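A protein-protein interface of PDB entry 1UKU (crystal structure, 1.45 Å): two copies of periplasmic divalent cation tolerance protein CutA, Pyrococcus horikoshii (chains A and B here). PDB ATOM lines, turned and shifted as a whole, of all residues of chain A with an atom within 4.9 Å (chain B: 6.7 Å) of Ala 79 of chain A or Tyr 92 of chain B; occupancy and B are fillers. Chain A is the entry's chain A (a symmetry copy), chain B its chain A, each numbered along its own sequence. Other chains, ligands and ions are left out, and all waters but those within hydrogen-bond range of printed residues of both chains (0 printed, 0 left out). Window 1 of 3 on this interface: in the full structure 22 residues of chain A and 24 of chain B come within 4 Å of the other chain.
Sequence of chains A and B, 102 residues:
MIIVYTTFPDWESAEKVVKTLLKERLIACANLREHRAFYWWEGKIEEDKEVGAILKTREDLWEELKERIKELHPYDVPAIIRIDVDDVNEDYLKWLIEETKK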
ATOM      1  N   TYR A   5       3.757  25.833  -5.920  1.00  0.00           N
ATOM      2  CA  TYR A   5       3.879  24.394  -6.165  1.00  0.00           C
ATOM      3  C   TYR A   5       2.990  23.648  -5.163  1.00  0.00           C
ATOM      4  O   TYR A   5       3.007  23.905  -3.966  1.00  0.00           O
ATOM      5  CB  TYR A   5       5.323  23.940  -6.005  1.00  0.00           C
ATOM      6  CG  TYR A   5       5.626  22.488  -6.318  1.00  0.00           C
ATOM      7  CD1 TYR A   5       5.491  22.001  -7.596  1.00  0.00           C
ATOM      8  CD2 TYR A   5       6.064  21.593  -5.321  1.00  0.00           C
ATOM      9  CE1 TYR A   5       5.782  20.664  -7.909  1.00  0.00           C
ATOM     10  CE2 TYR A   5       6.358  20.243  -5.632  1.00  0.00           C
ATOM     11  CZ  TYR A   5       6.220  19.804  -6.933  1.00  0.00           C
ATOM     12  OH  TYR A   5       6.529  18.495  -7.261  1.00  0.00           O
ATOM     13  N   THR A   6       2.222  22.690  -5.659  1.00  0.00           N
ATOM     14  CA  THR A   6       1.456  21.769  -4.840  1.00  0.00           C
ATOM     15  C   THR A   6       1.444  20.416  -5.545  1.00  0.00           C
ATOM     16  O   THR A   6       1.849  20.298  -6.690  1.00  0.00           O
ATOM     17  CB  THR A   6       0.046  22.334  -4.564  1.00  0.00           C
ATOM     18  OG1 THR A   6      -0.603  21.496  -3.589  1.00  0.00           O
ATOM     19  CG2 THR A   6      -0.842  22.385  -5.779  1.00  0.00           C
ATOM     20  N   THR A   7       1.043  19.380  -4.836  1.00  0.00           N
ATOM     21  CA  THR A   7       0.986  18.059  -5.409  1.00  0.00           C
ATOM     22  C   THR A   7      -0.368  17.478  -5.173  1.00  0.00           C
ATOM     23  O   THR A   7      -1.043  17.835  -4.216  1.00  0.00           O
ATOM     24  CB  THR A   7       2.055  17.120  -4.867  1.00  0.00           C
ATOM     25  OG1 THR A   7       1.727  16.715  -3.520  1.00  0.00           O
ATOM     26  CG2 THR A   7       3.413  17.776  -4.811  1.00  0.00           C
ATOM     27  N   VAL A  77      -3.356  17.624   4.592  1.00  0.00           N
ATOM     28  CA  VAL A  77      -2.197  18.488   4.785  1.00  0.00           C
ATOM     29  C   VAL A  77      -1.446  18.599   3.452  1.00  0.00           C
ATOM     30  O   VAL A  77      -0.462  17.895   3.220  1.00  0.00           O
ATOM     31  CB  VAL A  77      -1.269  17.980   5.917  1.00  0.00           C
ATOM     32  CG1 VAL A  77      -0.137  18.957   6.173  1.00  0.00           C
ATOM     33  CG2 VAL A  77      -2.057  17.770   7.222  1.00  0.00           C
ATOM     34  N   PRO A  78      -1.912  19.471   2.573  1.00  0.00           N
ATOM     35  CA  PRO A  78      -1.240  19.619   1.274  1.00  0.00           C
ATOM     36  C   PRO A  78      -0.012  20.468   1.418  1.00  0.00           C
ATOM     37  O   PRO A  78       0.095  21.250   2.361  1.00  0.00           O
ATOM     38  CB  PRO A  78      -2.269  20.353   0.436  1.00  0.00           C
ATOM     39  CG  PRO A  78      -3.047  21.150   1.423  1.00  0.00           C
ATOM     40  CD  PRO A  78      -3.056  20.373   2.706  1.00  0.00           C
ATOM     41  N   ALA A  79       0.905  20.337   0.466  1.00  0.00           N
ATOM     42  CA  ALA A  79       2.007  21.276   0.309  1.00  0.00           C
ATOM     43  C   ALA A  79       1.516  22.428  -0.567  1.00  0.00           C
ATOM     44  O   ALA A  79       1.076  22.226  -1.695  1.00  0.00           O
ATOM     45  CB  ALA A  79       3.193  20.614  -0.331  1.00  0.00           C
ATOM     46  N   ILE A  80       1.603  23.648  -0.057  1.00  0.00           N
ATOM     47  CA  ILE A  80       1.255  24.830  -0.826  1.00  0.00           C
ATOM     48  C   ILE A  80       2.407  25.824  -0.687  1.00  0.00           C
ATOM     49  O   ILE A  80       2.467  26.608   0.276  1.00  0.00           O
ATOM     50  CB  ILE A  80      -0.080  25.471  -0.354  1.00  0.00           C
ATOM     51  CG1 ILE A  80      -1.151  24.409  -0.196  1.00  0.00           C
ATOM     52  CG2 ILE A  80      -0.532  26.541  -1.369  1.00  0.00           C
ATOM     53  CD1 ILE A  80      -2.452  24.944   0.426  1.00  0.00           C
ATOM     54  N   ILE A  81       3.310  25.801  -1.661  1.00  0.00           N
ATOM     55  CA  ILE A  81       4.659  26.372  -1.567  1.00  0.00           C
ATOM     56  C   ILE A  81       4.800  27.539  -2.530  1.00  0.00           C
ATOM     57  O   ILE A  81       4.702  27.361  -3.734  1.00  0.00           O
ATOM     58  CB  ILE A  81       5.679  25.275  -1.878  1.00  0.00           C
ATOM     59  CG1 ILE A  81       5.745  24.285  -0.692  1.00  0.00           C
ATOM     60  CG2 ILE A  81       7.057  25.840  -2.163  1.00  0.00           C
ATOM     61  CD1 ILE A  81       6.505  22.974  -0.927  1.00  0.00           C
ATOM     62  N   MET B   1      11.200  27.205   5.308  1.00  0.00           N
ATOM     63  CA  MET B   1      11.637  25.925   4.705  1.00  0.00           C
ATOM     64  C   MET B   1      12.367  26.219   3.409  1.00  0.00           C
ATOM     65  O   MET B   1      12.346  27.336   2.894  1.00  0.00           O
ATOM     66  CB  MET B   1      10.436  25.015   4.457  1.00  0.00           C
ATOM     67  CG  MET B   1       9.486  25.452   3.378  1.00  0.00           C
ATOM     68  SD  MET B   1       8.261  24.179   2.933  1.00  0.00           S
ATOM     69  CE  MET B   1       9.256  23.094   1.894  1.00  0.00           C
ATOM     70  N   ALA B  28      12.109  15.981   4.732  1.00  0.00           N
ATOM     71  CA  ALA B  28      10.765  15.499   5.017  1.00  0.00           C
ATOM     72  C   ALA B  28      10.141  14.750   3.853  1.00  0.00           C
ATOM     73  O   ALA B  28       9.277  13.899   4.046  1.00  0.00           O
ATOM     74  CB  ALA B  28       9.863  16.639   5.407  1.00  0.00           C
ATOM     75  N   CYS B  29      10.547  15.101   2.640  1.00  0.00           N
ATOM     76  CA  CYS B  29      10.004  14.428   1.476  1.00  0.00           C
ATOM     77  C   CYS B  29      10.803  14.759   0.248  1.00  0.00           C
ATOM     78  O   CYS B  29      11.596  15.701   0.218  1.00  0.00           O
ATOM     79  CB  CYS B  29       8.567  14.804   1.297  1.00  0.00           C
ATOM     80  SG  CYS B  29       8.412  16.466   0.948  1.00  0.00           S
ATOM     81  N   LYS B  56      12.518  18.579   0.219  1.00  0.00           N
ATOM     82  CA  LYS B  56      11.916  19.619   1.066  1.00  0.00           C
ATOM     83  C   LYS B  56      12.447  19.442   2.473  1.00  0.00           C
ATOM     84  O   LYS B  56      12.388  18.359   3.033  1.00  0.00           O
ATOM     85  CB  LYS B  56      10.384  19.536   1.018  1.00  0.00           C
ATOM     86  CG  LYS B  56       9.826  19.564  -0.435  1.00  0.00           C
ATOM     87  CD  LYS B  56       8.340  19.184  -0.577  1.00  0.00           C
ATOM     88  CE  LYS B  56       8.054  18.124  -1.702  1.00  0.00           C
ATOM     89  NZ  LYS B  56       8.204  16.616  -1.329  1.00  0.00           N
ATOM     90  N   VAL B  88       4.620  29.237   2.859  1.00  0.00           N
ATOM     91  CA  VAL B  88       4.003  27.909   2.787  1.00  0.00           C
ATOM     92  C   VAL B  88       2.862  27.866   3.783  1.00  0.00           C
ATOM     93  O   VAL B  88       2.879  28.590   4.795  1.00  0.00           O
ATOM     94  CB  VAL B  88       5.074  26.800   3.043  1.00  0.00           C
ATOM     95  CG1 VAL B  88       5.714  27.018   4.381  1.00  0.00           C
ATOM     96  CG2 VAL B  88       4.518  25.417   2.898  1.00  0.00           C
ATOM     97  N   ASN B  89       1.861  27.044   3.507  1.00  0.00           N
ATOM     98  CA  ASN B  89       0.776  26.836   4.476  1.00  0.00           C
ATOM     99  C   ASN B  89       1.312  26.240   5.757  1.00  0.00           C
ATOM    100  O   ASN B  89       2.135  25.329   5.755  1.00  0.00           O
ATOM    101  CB  ASN B  89      -0.358  25.988   3.930  1.00  0.00           C
ATOM    102  CG  ASN B  89       0.113  24.647   3.389  1.00  0.00           C
ATOM    103  OD1 ASN B  89       1.070  24.574   2.591  1.00  0.00           O
ATOM    104  ND2 ASN B  89      -0.593  23.573   3.769  1.00  0.00           N
ATOM    105  N   GLU B  90       0.859  26.782   6.875  1.00  0.00           N
ATOM    106  CA  GLU B  90       1.393  26.371   8.162  1.00  0.00           C
ATOM    107  C   GLU B  90       1.256  24.899   8.508  1.00  0.00           C
ATOM    108  O   GLU B  90       2.158  24.359   9.125  1.00  0.00           O
ATOM    109  CB  GLU B  90       0.735  27.196   9.273  1.00  0.00           C
ATOM    110  CG  GLU B  90       1.058  26.701  10.670  1.00  0.00           C
ATOM    111  CD  GLU B  90       2.531  26.801  11.001  1.00  0.00           C
ATOM    112  OE1 GLU B  90       3.252  27.506  10.267  1.00  0.00           O
ATOM    113  OE2 GLU B  90       2.971  26.174  11.990  1.00  0.00           O
ATOM    114  N   ASP B  91       0.131  24.275   8.177  1.00  0.00           N
ATOM    115  CA  ASP B  91      -0.055  22.860   8.517  1.00  0.00           C
ATOM    116  C   ASP B  91       1.040  21.984   7.864  1.00  0.00           C
ATOM    117  O   ASP B  91       1.566  21.039   8.463  1.00  0.00           O
ATOM    118  CB  ASP B  91      -1.466  22.342   8.164  1.00  0.00           C
ATOM    119  CG  ASP B  91      -1.943  22.751   6.775  1.00  0.00           C
ATOM    120  OD1 ASP B  91      -1.797  23.938   6.366  1.00  0.00           O
ATOM    121  OD2 ASP B  91      -2.526  21.935   6.015  1.00  0.00           O
ATOM    122  N   TYR B  92       1.409  22.323   6.638  1.00  0.00           N
ATOM    123  CA  TYR B  92       2.471  21.602   5.981  1.00  0.00           C
ATOM    124  C   TYR B  92       3.826  21.874   6.645  1.00  0.00           C
ATOM    125  O   TYR B  92       4.623  20.960   6.864  1.00  0.00           O
ATOM    126  CB  TYR B  92       2.530  21.941   4.492  1.00  0.00           C
ATOM    127  CG  TYR B  92       3.568  21.121   3.788  1.00  0.00           C
ATOM    128  CD1 TYR B  92       3.293  19.830   3.404  1.00  0.00           C
ATOM    129  CD2 TYR B  92       4.844  21.617   3.567  1.00  0.00           C
ATOM    130  CE1 TYR B  92       4.261  19.064   2.769  1.00  0.00           C
ATOM    131  CE2 TYR B  92       5.808  20.855   2.964  1.00  0.00           C
ATOM    132  CZ  TYR B  92       5.498  19.600   2.545  1.00  0.00           C
ATOM    133  OH  TYR B  92       6.474  18.828   1.931  1.00  0.00           O
ATOM    134  N   LEU B  93       4.095  23.141   6.936  1.00  0.00           N
ATOM    135  CA  LEU B  93       5.341  23.497   7.575  1.00  0.00           C
ATOM    136  C   LEU B  93       5.490  22.771   8.905  1.00  0.00           C
ATOM    137  O   LEU B  93       6.542  22.246   9.207  1.00  0.00           O
ATOM    138  CB  LEU B  93       5.441  25.004   7.762  1.00  0.00           C
ATOM    139  CG  LEU B  93       6.752  25.506   8.343  1.00  0.00           C
ATOM    140  CD1 LEU B  93       7.958  25.119   7.479  1.00  0.00           C
ATOM    141  CD2 LEU B  93       6.586  27.007   8.456  1.00  0.00           C
ATOM    142  N   LYS B  94       4.415  22.696   9.678  1.00  0.00           N
ATOM    143  CA  LYS B  94       4.461  21.998  10.971  1.00  0.00           C
ATOM    144  C   LYS B  94       4.795  20.520  10.802  1.00  0.00           C
ATOM    145  O   LYS B  94       5.607  19.966  11.543  1.00  0.00           O
ATOM    146  CB  LYS B  94       3.141  22.163  11.715  1.00  0.00           C
ATOM    147  CG  LYS B  94       3.138  21.564  13.101  1.00  0.00           C
ATOM    148  CD  LYS B  94       4.244  22.181  13.953  1.00  0.00           C
ATOM    149  CE  LYS B  94       4.023  21.947  15.442  1.00  0.00           C
ATOM    150  NZ  LYS B  94       3.214  23.044  16.030  1.00  0.00           N
ATOM    151  N   TRP B  95       4.185  19.898   9.805  1.00  0.00           N
ATOM    152  CA  TRP B  95       4.460  18.510   9.490  1.00  0.00           C
ATOM    153  C   TRP B  95       5.926  18.329   9.089  1.00  0.00           C
ATOM    154  O   TRP B  95       6.590  17.443   9.548  1.00  0.00           O
ATOM    155  CB  TRP B  95       3.530  18.042   8.353  1.00  0.00           C
ATOM    156  CG  TRP B  95       3.857  16.668   7.859  1.00  0.00           C
ATOM    157  CD1 TRP B  95       3.496  15.479   8.429  1.00  0.00           C
ATOM    158  CD2 TRP B  95       4.635  16.336   6.711  1.00  0.00           C
ATOM    159  NE1 TRP B  95       4.009  14.425   7.707  1.00  0.00           N
ATOM    160  CE2 TRP B  95       4.698  14.926   6.633  1.00  0.00           C
ATOM    161  CE3 TRP B  95       5.285  17.085   5.729  1.00  0.00           C
ATOM    162  CZ2 TRP B  95       5.395  14.276   5.627  1.00  0.00           C
ATOM    163  CZ3 TRP B  95       5.965  16.416   4.724  1.00  0.00           C
ATOM    164  CH2 TRP B  95       6.024  15.052   4.689  1.00  0.00           C
ATOM    165  N   LEU B  96       6.427  19.201   8.229  1.00  0.00           N
ATOM    166  CA  LEU B  96       7.805  19.081   7.790  1.00  0.00           C
ATOM    167  C   LEU B  96       8.787  19.205   8.959  1.00  0.00           C
ATOM    168  O   LEU B  96       9.786  18.483   9.024  1.00  0.00           O
ATOM    169  CB  LEU B  96       8.069  20.141   6.713  1.00  0.00           C
ATOM    170  CG  LEU B  96       9.506  20.335   6.224  1.00  0.00           C
ATOM    171  CD1 LEU B  96       9.466  20.720   4.756  1.00  0.00           C
ATOM    172  CD2 LEU B  96      10.275  21.363   7.029  1.00  0.00           C
ATOM    173  N   ILE B  97       8.513  20.136   9.883  1.00  0.00           N
ATOM    174  CA  ILE B  97       9.362  20.282  11.072  1.00  0.00           C
ATOM    175  C   ILE B  97       9.279  19.018  11.949  1.00  0.00           C
ATOM    176  O   ILE B  97      10.286  18.502  12.440  1.00  0.00           O
ATOM    177  CB  ILE B  97       8.940  21.537  11.848  1.00  0.00           C
ATOM    178  CG1 ILE B  97       9.298  22.791  11.053  1.00  0.00           C
ATOM    179  CG2 ILE B  97       9.600  21.577  13.246  1.00  0.00           C
ATOM    180  CD1 ILE B  97       8.650  24.066  11.579  1.00  0.00           C
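The side-chain amide oxygen (OD1) of Asn 89 of chain B is in hydrogen-bond range of the backbone NH (N) of Ile 80 of chain A. ND2 of Asn 89 of chain B lies within hydrogen-bond range of O of Pro 78 of chain A (2.8 Å).
O of Ala 79 of chain A sits at hydrogen-bond distance from OG1 of Thr 6 of chain A, at 2.6 Å. OH of Tyr 92 of chain B is in hydrogen-bond range of SG of Cys 29 of chain B, 3.2 Å away. N of Tyr 5 of chain A lies within hydrogen-bond range of O of Ile 81 of chain A (2.8 Å). The side-chain amide nitrogen (ND2) of Asn 89 of chain B is in hydrogen-bond range of the side-chain carboxylate (OD1) of Asp 91 of chain B.
Among the printed residues, merely in contact across the chains: Val 77 of chain A with Asp 91 of chain B (3.5 Å), Val 77 of chain A with Tyr 92 of chain B (3.7 Å), Pro 78 of chain A with Asp 91 of chain B (3.7 Å), Pro 78 of chain A with Tyr 92 of chain B (3.3 Å), Ala 79 of chain A with Asn 89 of chain B (3.8 Å), Ala 79 of chain A with Tyr 92 of chain B (3.6 Å), Ile 80 of chain A with Val 88 of chain B (3.2 Å), Ile 81 of chain A with Met 1 of chain B (3.9 Å) and Ile 81 of chain A with Val 88 of chain B (3.96 Å).
Ala 79 of chain A touches two residues of chain B. Of chain A, only Val 77, Pro 78 and Ala 79 come within 4 Å of Tyr 92 of chain B. Of the printed residues of chain A, Val 88 of chain B touches Ile 80 (3.2 Å) and Ile 81 (3.96 Å). Printed residues of chain A within 4 Å of Asp 91 of chain B: Val 77 (3.5 Å) and Pro 78 (3.7 Å). The nearest residue of chain A that does not touch Tyr 92 of chain B is Ile 81 of chain A (4.5 Å).
Of the 14 printed residues of chain B, 5 touch a printed residue of chain A. Among the printed residues, 11 pairs touch across the chains.
No position is printed for both chains.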
